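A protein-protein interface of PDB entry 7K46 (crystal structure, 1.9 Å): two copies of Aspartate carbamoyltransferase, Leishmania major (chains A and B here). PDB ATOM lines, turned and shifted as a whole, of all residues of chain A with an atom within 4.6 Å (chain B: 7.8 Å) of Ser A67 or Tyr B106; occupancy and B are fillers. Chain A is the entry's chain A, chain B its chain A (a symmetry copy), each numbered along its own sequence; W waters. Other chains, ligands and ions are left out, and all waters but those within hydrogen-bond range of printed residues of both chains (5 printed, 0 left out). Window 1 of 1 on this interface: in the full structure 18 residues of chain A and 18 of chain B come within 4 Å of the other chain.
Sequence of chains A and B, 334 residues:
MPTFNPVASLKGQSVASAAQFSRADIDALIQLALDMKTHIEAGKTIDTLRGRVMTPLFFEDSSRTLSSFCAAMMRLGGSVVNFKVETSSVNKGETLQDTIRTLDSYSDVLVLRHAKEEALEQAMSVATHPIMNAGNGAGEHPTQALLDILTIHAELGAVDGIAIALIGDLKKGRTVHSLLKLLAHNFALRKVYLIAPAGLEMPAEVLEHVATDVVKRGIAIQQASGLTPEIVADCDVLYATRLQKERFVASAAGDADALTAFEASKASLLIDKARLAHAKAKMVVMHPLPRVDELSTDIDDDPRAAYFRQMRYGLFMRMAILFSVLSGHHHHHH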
ATOM      1  N   SER A  63      -6.699   6.174  27.867  1.00  0.00           N
ATOM      2  CA  SER A  63      -5.881   6.224  26.663  1.00  0.00           C
ATOM      3  C   SER A  63      -6.723   6.519  25.434  1.00  0.00           C
ATOM      4  O   SER A  63      -6.251   7.204  24.520  1.00  0.00           O
ATOM      5  CB  SER A  63      -5.118   4.914  26.485  1.00  0.00           C
ATOM      6  OG  SER A  63      -4.145   4.758  27.510  1.00  0.00           O
ATOM      7  N   ARG A  64      -7.966   6.020  25.398  1.00  0.00           N
ATOM      8  CA  ARG A  64      -8.863   6.307  24.273  1.00  0.00           C
ATOM      9  C   ARG A  64      -9.106   7.811  24.118  1.00  0.00           C
ATOM     10  O   ARG A  64      -8.973   8.365  23.020  1.00  0.00           O
ATOM     11  CB  ARG A  64     -10.184   5.555  24.461  1.00  0.00           C
ATOM     12  CG  ARG A  64     -11.315   5.963  23.497  1.00  0.00           C
ATOM     13  CD  ARG A  64     -12.547   5.037  23.654  1.00  0.00           C
ATOM     14  NE  ARG A  64     -12.255   3.685  23.182  1.00  0.00           N
ATOM     15  CZ  ARG A  64     -11.975   2.655  23.969  1.00  0.00           C
ATOM     16  NH1 ARG A  64     -12.013   2.759  25.295  1.00  0.00           N
ATOM     17  NH2 ARG A  64     -11.650   1.493  23.417  1.00  0.00           N
ATOM     18  N   THR A  65      -9.466   8.497  25.204  1.00  0.00           N
ATOM     19  CA  THR A  65      -9.741   9.929  25.093  1.00  0.00           C
ATOM     20  C   THR A  65      -8.447  10.734  24.916  1.00  0.00           C
ATOM     21  O   THR A  65      -8.393  11.671  24.106  1.00  0.00           O
ATOM     22  CB  THR A  65     -10.531  10.402  26.317  1.00  0.00           C
ATOM     23  OG1 THR A  65     -11.820   9.755  26.322  1.00  0.00           O
ATOM     24  CG2 THR A  65     -10.745  11.901  26.276  1.00  0.00           C
ATOM     25  N   LEU A  66      -7.398  10.374  25.653  1.00  0.00           N
ATOM     26  CA  LEU A  66      -6.127  11.090  25.545  1.00  0.00           C
ATOM     27  C   LEU A  66      -5.577  11.029  24.122  1.00  0.00           C
ATOM     28  O   LEU A  66      -5.223  12.061  23.535  1.00  0.00           O
ATOM     29  CB  LEU A  66      -5.122  10.500  26.538  1.00  0.00           C
ATOM     30  CG  LEU A  66      -3.682  11.027  26.478  1.00  0.00           C
ATOM     31  CD1 LEU A  66      -3.669  12.523  26.721  1.00  0.00           C
ATOM     32  CD2 LEU A  66      -2.812  10.301  27.503  1.00  0.00           C
ATOM     33  N   SER A  67      -5.490   9.826  23.544  1.00  0.00           N
ATOM     34  CA  SER A  67      -4.862   9.717  22.227  1.00  0.00           C
ATOM     35  C   SER A  67      -5.666  10.465  21.170  1.00  0.00           C
ATOM     36  O   SER A  67      -5.090  11.037  20.238  1.00  0.00           O
ATOM     37  CB  SER A  67      -4.685   8.245  21.846  1.00  0.00           C
ATOM     38  OG  SER A  67      -5.934   7.571  21.795  1.00  0.00           O
ATOM     39  N   SER A  68      -6.989  10.515  21.324  1.00  0.00           N
ATOM     40  CA  SER A  68      -7.827  11.257  20.381  1.00  0.00           C
ATOM     41  C   SER A  68      -7.514  12.754  20.414  1.00  0.00           C
ATOM     42  O   SER A  68      -7.361  13.390  19.362  1.00  0.00           O
ATOM     43  CB  SER A  68      -9.304  11.006  20.699  1.00  0.00           C
ATOM     44  OG  SER A  68     -10.149  11.551  19.691  1.00  0.00           O
ATOM     45  N   PHE A  69      -7.421  13.339  21.616  1.00  0.00           N
ATOM     46  CA  PHE A  69      -7.024  14.747  21.727  1.00  0.00           C
ATOM     47  C   PHE A  69      -5.646  14.987  21.116  1.00  0.00           C
ATOM     48  O   PHE A  69      -5.438  15.980  20.406  1.00  0.00           O
ATOM     49  CB  PHE A  69      -7.014  15.199  23.196  1.00  0.00           C
ATOM     50  CG  PHE A  69      -8.341  15.707  23.687  1.00  0.00           C
ATOM     51  CD1 PHE A  69      -8.782  16.975  23.332  1.00  0.00           C
ATOM     52  CD2 PHE A  69      -9.126  14.930  24.525  1.00  0.00           C
ATOM     53  CE1 PHE A  69     -10.019  17.460  23.784  1.00  0.00           C
ATOM     54  CE2 PHE A  69     -10.356  15.403  24.987  1.00  0.00           C
ATOM     55  CZ  PHE A  69     -10.798  16.674  24.614  1.00  0.00           C
ATOM     56  N   CYS A  70      -4.690  14.104  21.403  1.00  0.00           N
ATOM     57  CA  CYS A  70      -3.340  14.278  20.866  1.00  0.00           C
ATOM     58  C   CYS A  70      -3.322  14.150  19.352  1.00  0.00           C
ATOM     59  O   CYS A  70      -2.673  14.946  18.664  1.00  0.00           O
ATOM     60  CB  CYS A  70      -2.386  13.265  21.491  1.00  0.00           C
ATOM     61  SG  CYS A  70      -2.172  13.582  23.262  1.00  0.00           S
ATOM     62  N   ALA A  71      -4.022  13.148  18.816  1.00  0.00           N
ATOM     63  CA  ALA A  71      -4.055  12.977  17.365  1.00  0.00           C
ATOM     64  C   ALA A  71      -4.752  14.152  16.690  1.00  0.00           C
ATOM     65  O   ALA A  71      -4.315  14.618  15.628  1.00  0.00           O
ATOM     66  CB  ALA A  71      -4.752  11.667  17.010  1.00  0.00           C
ATOM     67  N   ARG A  75      -2.964  16.452  13.844  1.00  0.00           N
ATOM     68  CA  ARG A  75      -3.537  16.536  12.505  1.00  0.00           C
ATOM     69  C   ARG A  75      -3.993  17.950  12.148  1.00  0.00           C
ATOM     70  O   ARG A  75      -4.446  18.173  11.021  1.00  0.00           O
ATOM     71  CB  ARG A  75      -4.700  15.552  12.377  1.00  0.00           C
ATOM     72  CG  ARG A  75      -4.263  14.078  12.372  1.00  0.00           C
ATOM     73  CD  ARG A  75      -5.454  13.183  12.068  1.00  0.00           C
ATOM     74  NE  ARG A  75      -5.079  11.779  11.960  1.00  0.00           N
ATOM     75  CZ  ARG A  75      -4.623  11.209  10.855  1.00  0.00           C
ATOM     76  NH1 ARG A  75      -4.411  11.914   9.748  1.00  0.00           N
ATOM     77  NH2 ARG A  75      -4.355   9.905  10.864  1.00  0.00           N
ATOM     78  N   ARG A 312     -13.823   7.521  15.443  1.00  0.00           N
ATOM     79  CA  ARG A 312     -13.262   8.376  14.403  1.00  0.00           C
ATOM     80  C   ARG A 312     -14.032   9.690  14.305  1.00  0.00           C
ATOM     81  O   ARG A 312     -13.435  10.756  14.094  1.00  0.00           O
ATOM     82  CB  ARG A 312     -13.250   7.630  13.069  1.00  0.00           C
ATOM     83  CG  ARG A 312     -12.580   8.403  11.930  1.00  0.00           C
ATOM     84  CD  ARG A 312     -11.957   7.453  10.912  1.00  0.00           C
ATOM     85  NE  ARG A 312     -11.300   8.135   9.805  1.00  0.00           N
ATOM     86  CZ  ARG A 312     -10.005   8.423   9.772  1.00  0.00           C
ATOM     87  NH1 ARG A 312      -9.228   8.221  10.827  1.00  0.00           N
ATOM     88  NH2 ARG A 312      -9.475   8.921   8.654  1.00  0.00           N
ATOM     89  N   LEU A 315     -12.382  11.844  16.773  1.00  0.00           N
ATOM     90  CA  LEU A 315     -11.206  12.545  16.262  1.00  0.00           C
ATOM     91  C   LEU A 315     -11.599  13.847  15.566  1.00  0.00           C
ATOM     92  O   LEU A 315     -11.036  14.912  15.844  1.00  0.00           O
ATOM     93  CB  LEU A 315     -10.428  11.638  15.297  1.00  0.00           C
ATOM     94  CG  LEU A 315      -9.316  12.334  14.493  1.00  0.00           C
ATOM     95  CD1 LEU A 315      -8.137  12.733  15.390  1.00  0.00           C
ATOM     96  CD2 LEU A 315      -8.832  11.432  13.349  1.00  0.00           C
ATOM     97  N   GLY B  51       1.467  14.912   8.519  1.00  0.00           N
ATOM     98  CA  GLY B  51       0.057  14.648   8.716  1.00  0.00           C
ATOM     99  C   GLY B  51      -0.330  13.187   8.861  1.00  0.00           C
ATOM    100  O   GLY B  51      -1.524  12.901   9.014  1.00  0.00           O
ATOM    101  N   ARG B  52       0.623  12.257   8.806  1.00  0.00           N
ATOM    102  CA  ARG B  52       0.348  10.848   9.053  1.00  0.00           C
ATOM    103  C   ARG B  52       0.750  10.497  10.483  1.00  0.00           C
ATOM    104  O   ARG B  52       1.710  11.045  11.024  1.00  0.00           O
ATOM    105  CB  ARG B  52       1.097   9.946   8.066  1.00  0.00           C
ATOM    106  CG  ARG B  52       0.980  10.379   6.604  1.00  0.00           C
ATOM    107  CD  ARG B  52      -0.471  10.495   6.128  1.00  0.00           C
ATOM    108  NE  ARG B  52      -0.523  11.234   4.866  1.00  0.00           N
ATOM    109  CZ  ARG B  52      -1.475  12.087   4.514  1.00  0.00           C
ATOM    110  NH1 ARG B  52      -2.533  12.304   5.282  1.00  0.00           N
ATOM    111  NH2 ARG B  52      -1.365  12.744   3.359  1.00  0.00           N
ATOM    112  N   VAL B  53       0.014   9.566  11.085  1.00  0.00           N
ATOM    113  CA  VAL B  53       0.113   9.284  12.515  1.00  0.00           C
ATOM    114  C   VAL B  53       0.523   7.832  12.728  1.00  0.00           C
ATOM    115  O   VAL B  53      -0.108   6.919  12.186  1.00  0.00           O
ATOM    116  CB  VAL B  53      -1.222   9.569  13.225  1.00  0.00           C
ATOM    117  CG1 VAL B  53      -1.211   9.000  14.663  1.00  0.00           C
ATOM    118  CG2 VAL B  53      -1.502  11.068  13.223  1.00  0.00           C
ATOM    119  N   MET B  54       1.561   7.629  13.535  1.00  0.00           N
ATOM    120  CA  MET B  54       1.952   6.316  14.029  1.00  0.00           C
ATOM    121  C   MET B  54       1.513   6.198  15.482  1.00  0.00           C
ATOM    122  O   MET B  54       1.739   7.127  16.271  1.00  0.00           O
ATOM    123  CB  MET B  54       3.475   6.137  13.936  1.00  0.00           C
ATOM    124  CG  MET B  54       4.035   4.983  14.811  1.00  0.00           C
ATOM    125  SD  MET B  54       5.851   4.973  14.885  1.00  0.00           S
ATOM    126  CE  MET B  54       6.239   4.368  13.241  1.00  0.00           C
ATOM    127  N   THR B  55       0.912   5.062  15.844  1.00  0.00           N
ATOM    128  CA  THR B  55       0.732   4.735  17.262  1.00  0.00           C
ATOM    129  C   THR B  55       1.502   3.467  17.597  1.00  0.00           C
ATOM    130  O   THR B  55       1.171   2.387  17.072  1.00  0.00           O
ATOM    131  CB  THR B  55      -0.740   4.548  17.653  1.00  0.00           C
ATOM    132  OG1 THR B  55      -1.476   5.744  17.380  1.00  0.00           O
ATOM    133  CG2 THR B  55      -0.836   4.255  19.151  1.00  0.00           C
ATOM    134  N   PRO B  56       2.490   3.530  18.484  1.00  0.00           N
ATOM    135  CA  PRO B  56       3.082   2.301  19.023  1.00  0.00           C
ATOM    136  C   PRO B  56       2.252   1.763  20.176  1.00  0.00           C
ATOM    137  O   PRO B  56       1.732   2.519  21.004  1.00  0.00           O
ATOM    138  CB  PRO B  56       4.470   2.753  19.511  1.00  0.00           C
ATOM    139  CG  PRO B  56       4.591   4.231  19.091  1.00  0.00           C
ATOM    140  CD  PRO B  56       3.187   4.727  18.976  1.00  0.00           C
ATOM    141  N   LEU B  57       2.133   0.438  20.219  1.00  0.00           N
ATOM    142  CA  LEU B  57       1.409  -0.259  21.278  1.00  0.00           C
ATOM    143  C   LEU B  57       2.366  -1.321  21.803  1.00  0.00           C
ATOM    144  O   LEU B  57       2.509  -2.388  21.196  1.00  0.00           O
ATOM    145  CB  LEU B  57       0.100  -0.861  20.760  1.00  0.00           C
ATOM    146  CG  LEU B  57      -0.882  -1.366  21.820  1.00  0.00           C
ATOM    147  CD1 LEU B  57      -1.464  -0.191  22.625  1.00  0.00           C
ATOM    148  CD2 LEU B  57      -1.987  -2.199  21.175  1.00  0.00           C
ATOM    149  N   VAL B  80       3.688  11.036  15.919  1.00  0.00           N
ATOM    150  CA  VAL B  80       3.581   9.849  16.764  1.00  0.00           C
ATOM    151  C   VAL B  80       2.671  10.150  17.945  1.00  0.00           C
ATOM    152  O   VAL B  80       2.879  11.135  18.662  1.00  0.00           O
ATOM    153  CB  VAL B  80       4.955   9.380  17.277  1.00  0.00           C
ATOM    154  CG1 VAL B  80       4.780   8.151  18.181  1.00  0.00           C
ATOM    155  CG2 VAL B  80       5.875   9.081  16.100  1.00  0.00           C
ATOM    156  N   VAL B  81       1.690   9.281  18.170  1.00  0.00           N
ATOM    157  CA  VAL B  81       0.783   9.378  19.306  1.00  0.00           C
ATOM    158  C   VAL B  81       1.042   8.179  20.210  1.00  0.00           C
ATOM    159  O   VAL B  81       0.995   7.035  19.748  1.00  0.00           O
ATOM    160  CB  VAL B  81      -0.687   9.402  18.847  1.00  0.00           C
ATOM    161  CG1 VAL B  81      -1.634   9.305  20.059  1.00  0.00           C
ATOM    162  CG2 VAL B  81      -0.968  10.673  18.025  1.00  0.00           C
ATOM    163  N   ASN B  82       1.306   8.440  21.488  1.00  0.00           N
ATOM    164  CA  ASN B  82       1.498   7.365  22.456  1.00  0.00           C
ATOM    165  C   ASN B  82       0.155   6.769  22.864  1.00  0.00           C
ATOM    166  O   ASN B  82      -0.876   7.445  22.852  1.00  0.00           O
ATOM    167  CB  ASN B  82       2.215   7.878  23.708  1.00  0.00           C
ATOM    168  CG  ASN B  82       3.381   8.785  23.382  1.00  0.00           C
ATOM    169  OD1 ASN B  82       4.259   8.433  22.594  1.00  0.00           O
ATOM    170  ND2 ASN B  82       3.393   9.970  23.990  1.00  0.00           N
ATOM    171  N   PHE B  83       0.173   5.491  23.242  1.00  0.00           N
ATOM    172  CA  PHE B  83      -1.028   4.833  23.758  1.00  0.00           C
ATOM    173  C   PHE B  83      -0.585   3.897  24.877  1.00  0.00           C
ATOM    174  O   PHE B  83      -0.054   2.816  24.611  1.00  0.00           O
ATOM    175  CB  PHE B  83      -1.762   4.078  22.660  1.00  0.00           C
ATOM    176  CG  PHE B  83      -3.163   3.690  23.023  1.00  0.00           C
ATOM    177  CD1 PHE B  83      -3.408   2.580  23.828  1.00  0.00           C
ATOM    178  CD2 PHE B  83      -4.241   4.427  22.552  1.00  0.00           C
ATOM    179  CE1 PHE B  83      -4.701   2.215  24.154  1.00  0.00           C
ATOM    180  CE2 PHE B  83      -5.540   4.066  22.872  1.00  0.00           C
ATOM    181  CZ  PHE B  83      -5.774   2.963  23.679  1.00  0.00           C
ATOM    182  N   LYS B  84      -0.804   4.317  26.118  1.00  0.00           N
ATOM    183  CA  LYS B  84      -0.413   3.520  27.275  1.00  0.00           C
ATOM    184  C   LYS B  84      -1.308   2.296  27.388  1.00  0.00           C
ATOM    185  O   LYS B  84      -2.539   2.416  27.440  1.00  0.00           O
ATOM    186  CB  LYS B  84      -0.499   4.356  28.550  1.00  0.00           C
ATOM    187  N   THR B  99      -8.681  -2.634  21.411  1.00  0.00           N
ATOM    188  CA  THR B  99      -7.632  -1.626  21.486  1.00  0.00           C
ATOM    189  C   THR B  99      -7.105  -1.282  20.100  1.00  0.00           C
ATOM    190  O   THR B  99      -6.895  -0.102  19.784  1.00  0.00           O
ATOM    191  CB  THR B  99      -6.502  -2.112  22.393  1.00  0.00           C
ATOM    192  OG1 THR B  99      -7.024  -2.323  23.712  1.00  0.00           O
ATOM    193  CG2 THR B  99      -5.379  -1.071  22.447  1.00  0.00           C
ATOM    194  N   ILE B 100      -6.883  -2.302  19.261  1.00  0.00           N
ATOM    195  CA  ILE B 100      -6.442  -2.070  17.885  1.00  0.00           C
ATOM    196  C   ILE B 100      -7.449  -1.199  17.139  1.00  0.00           C
ATOM    197  O   ILE B 100      -7.074  -0.246  16.445  1.00  0.00           O
ATOM    198  CB  ILE B 100      -6.209  -3.414  17.167  1.00  0.00           C
ATOM    199  CG1 ILE B 100      -5.043  -4.172  17.824  1.00  0.00           C
ATOM    200  CG2 ILE B 100      -5.974  -3.211  15.655  1.00  0.00           C
ATOM    201  CD1 ILE B 100      -3.689  -3.448  17.731  1.00  0.00           C
ATOM    202  N   ARG B 101      -8.742  -1.525  17.252  1.00  0.00           N
ATOM    203  CA  ARG B 101      -9.769  -0.700  16.612  1.00  0.00           C
ATOM    204  C   ARG B 101      -9.689   0.743  17.090  1.00  0.00           C
ATOM    205  O   ARG B 101      -9.914   1.683  16.315  1.00  0.00           O
ATOM    206  CB  ARG B 101     -11.165  -1.254  16.900  1.00  0.00           C
ATOM    207  CG  ARG B 101     -11.353  -2.737  16.606  1.00  0.00           C
ATOM    208  CD  ARG B 101     -12.421  -2.927  15.583  1.00  0.00           C
ATOM    209  NE  ARG B 101     -12.908  -4.299  15.496  1.00  0.00           N
ATOM    210  CZ  ARG B 101     -13.549  -4.764  14.436  1.00  0.00           C
ATOM    211  NH1 ARG B 101     -13.729  -4.012  13.361  1.00  0.00           N
ATOM    212  NH2 ARG B 101     -14.013  -6.011  14.451  1.00  0.00           N
ATOM    213  N   THR B 102      -9.403   0.938  18.378  1.00  0.00           N
ATOM    214  CA  THR B 102      -9.256   2.289  18.904  1.00  0.00           C
ATOM    215  C   THR B 102      -8.100   3.017  18.216  1.00  0.00           C
ATOM    216  O   THR B 102      -8.247   4.169  17.790  1.00  0.00           O
ATOM    217  CB  THR B 102      -9.066   2.219  20.426  1.00  0.00           C
ATOM    218  OG1 THR B 102     -10.218   1.590  21.013  1.00  0.00           O
ATOM    219  CG2 THR B 102      -8.912   3.620  21.030  1.00  0.00           C
ATOM    220  N   LEU B 103      -6.956   2.340  18.052  1.00  0.00           N
ATOM    221  CA  LEU B 103      -5.828   2.950  17.347  1.00  0.00           C
ATOM    222  C   LEU B 103      -6.177   3.267  15.895  1.00  0.00           C
ATOM    223  O   LEU B 103      -5.781   4.316  15.368  1.00  0.00           O
ATOM    224  CB  LEU B 103      -4.607   2.029  17.408  1.00  0.00           C
ATOM    225  CG  LEU B 103      -3.650   2.166  18.591  1.00  0.00           C
ATOM    226  CD1 LEU B 103      -4.367   1.943  19.916  1.00  0.00           C
ATOM    227  CD2 LEU B 103      -2.463   1.200  18.440  1.00  0.00           C
ATOM    228  N   ASP B 104      -6.907   2.367  15.225  1.00  0.00           N
ATOM    229  CA  ASP B 104      -7.266   2.581  13.822  1.00  0.00           C
ATOM    230  C   ASP B 104      -8.207   3.758  13.630  1.00  0.00           C
ATOM    231  O   ASP B 104      -8.384   4.220  12.493  1.00  0.00           O
ATOM    232  CB  ASP B 104      -7.945   1.346  13.225  1.00  0.00           C
ATOM    233  CG  ASP B 104      -6.965   0.313  12.726  1.00  0.00           C
ATOM    234  OD1 ASP B 104      -5.854   0.669  12.277  1.00  0.00           O
ATOM    235  OD2 ASP B 104      -7.324  -0.880  12.773  1.00  0.00           O
ATOM    236  N   SER B 105      -8.864   4.217  14.694  1.00  0.00           N
ATOM    237  CA  SER B 105      -9.776   5.336  14.535  1.00  0.00           C
ATOM    238  C   SER B 105      -9.035   6.626  14.188  1.00  0.00           C
ATOM    239  O   SER B 105      -9.637   7.541  13.618  1.00  0.00           O
ATOM    240  CB  SER B 105     -10.612   5.516  15.802  1.00  0.00           C
ATOM    241  OG  SER B 105      -9.819   6.059  16.849  1.00  0.00           O
ATOM    242  N   TYR B 106      -7.746   6.718  14.496  1.00  0.00           N
ATOM    243  CA  TYR B 106      -7.038   7.962  14.238  1.00  0.00           C
ATOM    244  C   TYR B 106      -5.648   7.780  13.632  1.00  0.00           C
ATOM    245  O   TYR B 106      -5.014   8.789  13.302  1.00  0.00           O
ATOM    246  CB  TYR B 106      -6.943   8.785  15.545  1.00  0.00           C
ATOM    247  CG  TYR B 106      -6.087   8.102  16.572  1.00  0.00           C
ATOM    248  CD1 TYR B 106      -4.696   8.209  16.515  1.00  0.00           C
ATOM    249  CD2 TYR B 106      -6.652   7.308  17.569  1.00  0.00           C
ATOM    250  CE1 TYR B 106      -3.882   7.560  17.429  1.00  0.00           C
ATOM    251  CE2 TYR B 106      -5.840   6.644  18.496  1.00  0.00           C
ATOM    252  CZ  TYR B 106      -4.451   6.775  18.408  1.00  0.00           C
ATOM    253  OH  TYR B 106      -3.617   6.132  19.302  1.00  0.00           O
ATOM    254  N   SER B 107      -5.153   6.548  13.471  1.00  0.00           N
ATOM    255  CA  SER B 107      -3.775   6.281  13.060  1.00  0.00           C
ATOM    256  C   SER B 107      -3.691   5.910  11.581  1.00  0.00           C
ATOM    257  O   SER B 107      -4.659   5.448  10.971  1.00  0.00           O
ATOM    258  CB  SER B 107      -3.153   5.132  13.874  1.00  0.00           C
ATOM    259  OG  SER B 107      -3.153   5.376  15.270  1.00  0.00           O
ATOM    260  N   ASP B 108      -2.489   6.085  11.023  1.00  0.00           N
ATOM    261  CA  ASP B 108      -2.144   5.579   9.699  1.00  0.00           C
ATOM    262  C   ASP B 108      -1.299   4.313   9.743  1.00  0.00           C
ATOM    263  O   ASP B 108      -1.308   3.545   8.780  1.00  0.00           O
ATOM    264  CB  ASP B 108      -1.378   6.643   8.906  1.00  0.00           C
ATOM    265  CG  ASP B 108      -2.220   7.866   8.627  1.00  0.00           C
ATOM    266  OD1 ASP B 108      -2.973   7.866   7.624  1.00  0.00           O
ATOM    267  OD2 ASP B 108      -2.154   8.807   9.440  1.00  0.00           O
ATOM    268  N   VAL B 109      -0.538   4.105  10.810  1.00  0.00           N
ATOM    269  CA  VAL B 109       0.297   2.916  10.942  1.00  0.00           C
ATOM    270  C   VAL B 109       0.392   2.582  12.422  1.00  0.00           C
ATOM    271  O   VAL B 109       0.461   3.477  13.273  1.00  0.00           O
ATOM    272  CB  VAL B 109       1.695   3.110  10.293  1.00  0.00           C
ATOM    273  CG1 VAL B 109       2.488   4.233  10.972  1.00  0.00           C
ATOM    274  CG2 VAL B 109       2.497   1.784  10.295  1.00  0.00           C
ATOM    275  N   LEU B 110       0.351   1.284  12.732  1.00  0.00           N
ATOM    276  CA  LEU B 110       0.495   0.801  14.096  1.00  0.00           C
ATOM    277  C   LEU B 110       1.822   0.068  14.227  1.00  0.00           C
ATOM    278  O   LEU B 110       2.312  -0.523  13.260  1.00  0.00           O
ATOM    279  CB  LEU B 110      -0.659  -0.142  14.476  1.00  0.00           C
ATOM    280  CG  LEU B 110      -2.097   0.270  14.134  1.00  0.00           C
ATOM    281  CD1 LEU B 110      -3.086  -0.712  14.782  1.00  0.00           C
ATOM    282  CD2 LEU B 110      -2.365   1.675  14.617  1.00  0.00           C
ATOM    283  N   HIS B 129      -5.309  -0.576   9.235  1.00  0.00           N
ATOM    284  CA  HIS B 129      -4.089   0.074   8.795  1.00  0.00           C
ATOM    285  C   HIS B 129      -2.926  -0.892   8.987  1.00  0.00           C
ATOM    286  O   HIS B 129      -3.041  -1.869   9.735  1.00  0.00           O
ATOM    287  CB  HIS B 129      -3.837   1.377   9.573  1.00  0.00           C
ATOM    288  CG  HIS B 129      -4.890   2.419   9.349  1.00  0.00           C
ATOM    289  ND1 HIS B 129      -5.959   2.593  10.202  1.00  0.00           N
ATOM    290  CD2 HIS B 129      -5.069   3.299   8.335  1.00  0.00           C
ATOM    291  CE1 HIS B 129      -6.737   3.555   9.737  1.00  0.00           C
ATOM    292  NE2 HIS B 129      -6.218   4.001   8.605  1.00  0.00           N
HETATM  293  O   HOH W   1      -6.673   7.322  10.374  1.00  0.00           O
HETATM  294  O   HOH W   2      -3.994  10.434   7.312  1.00  0.00           O
HETATM  295  O   HOH W   3      -1.673   6.767  26.651  1.00  0.00           O
HETATM  296  O   HOH W   4      -3.631  14.409   8.502  1.00  0.00           O
HETATM  297  O   HOH W   5       0.660  11.487  22.381  1.00  0.00           O
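The backbone carbonyl oxygen (O) of Tyr B106 lies within hydrogen-bond range of the guanidinium group (NH2) of Arg A75, 2.8 Å away. The guanidinium group of Arg A312 lies within hydrogen-bond range of the backbone carbonyl oxygen of Ser B105 (2.9 Å). The side-chain hydroxyl (OG1) of Thr B102 is in hydrogen-bond range of the guanidinium group (NH2) of Arg A64 (2.8 Å). The side-chain hydroxyl of Ser A63 is in hydrogen-bond range of the backbone carbonyl oxygen of Lys B84 (2.8 Å). NH1 of Arg A75 sits at hydrogen-bond distance from O of Gly B51, 3.1 Å away. OD2 of Asp B108 is in salt-bridge range of NH2 of Arg A75 (2.8 Å).
Hydrophobic or aromatic side chains of chain A that line the printed part of chain B: Ala A71 and Leu A315. Hydrophobic or aromatic side chains of chain B within 4 Å of the printed part of chain A: Val B53, Val B81, Phe B83 and Tyr B106.
The backbone carbonyl oxygen (O) of Met B54 lies within hydrogen-bond range of the backbone NH (N) of Val B81 (2.9 Å). O of Thr B102 is in hydrogen-bond range of OG of Ser B105 (2.6 Å). OG1 of Thr B55 sits at hydrogen-bond distance from OH of Tyr B106 (2.9 Å). The backbone carbonyl oxygen (O) of Ser A63 is in hydrogen-bond range of the side-chain hydroxyl (OG) of Ser A67 (2.8 Å). N of Val B109 sits at hydrogen-bond distance from O of Val B53 (3.2 Å). OG of Ser A67 lies within hydrogen-bond range of O of Arg A64 (3.4 Å).
Among the printed residues, merely in contact across the chains: Ser A63 with Phe B83 (3.5 Å), Ser A67 with Val B81 (3.7 Å), Ser A67 with Phe B83 (3.7 Å), Ser A67 with Tyr B106 (3.4 Å), Ala A71 with Val B81 (3.9 Å), Ala A71 with Tyr B106 (3.5 Å), Arg A75 with Val B53 (3.9 Å), Leu A315 with Ser B105 (3.98 Å) and Leu A315 with Tyr B106 (3.9 Å).
Water W4 lies within hydrogen-bond range of O of Gly B51 (2.6 Å) and NH1 of Arg A75 (2.9 Å). Water W3 lies within hydrogen-bond range of N of Lys B84 (2.7 Å) and OG of Ser A63 (3.3 Å). Water W1 lies within hydrogen-bond range of the guanidinium group (NH1) of Arg A312 and the backbone carbonyl oxygen (O) of Ser B107. Water W2 lies within hydrogen-bond range of the side-chain carboxylate of Asp B108 (2.8 Å), the guanidinium group of Arg A75 (2.9 Å) and the guanidinium group of Arg B52 (3.1 Å). Water W5 lies within hydrogen-bond range of N of Asn B82 (3.2 Å) and SG of Cys A70 (3.6 Å).
Of the printed residues of chain B, Ser A63 touches Phe B83 (3.5 Å) and Lys B84 (2.8 Å). Of the printed residues of chain B, Arg A75 touches Gly B51, Val B53, Tyr B106 and Asp B108. Printed residues of chain B within 4 Å of Leu A315: Ser B105 and Tyr B106. Ile B100 touches none of the printed residues of chain A. Asp B104 touches none of the printed residues of chain A. Tyr B106 touches four residues of chain A.
No position is printed for both chains. Of the 15 pairs that touch across the chains among the printed residues, none has its exchanged pair printed and touching as well.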
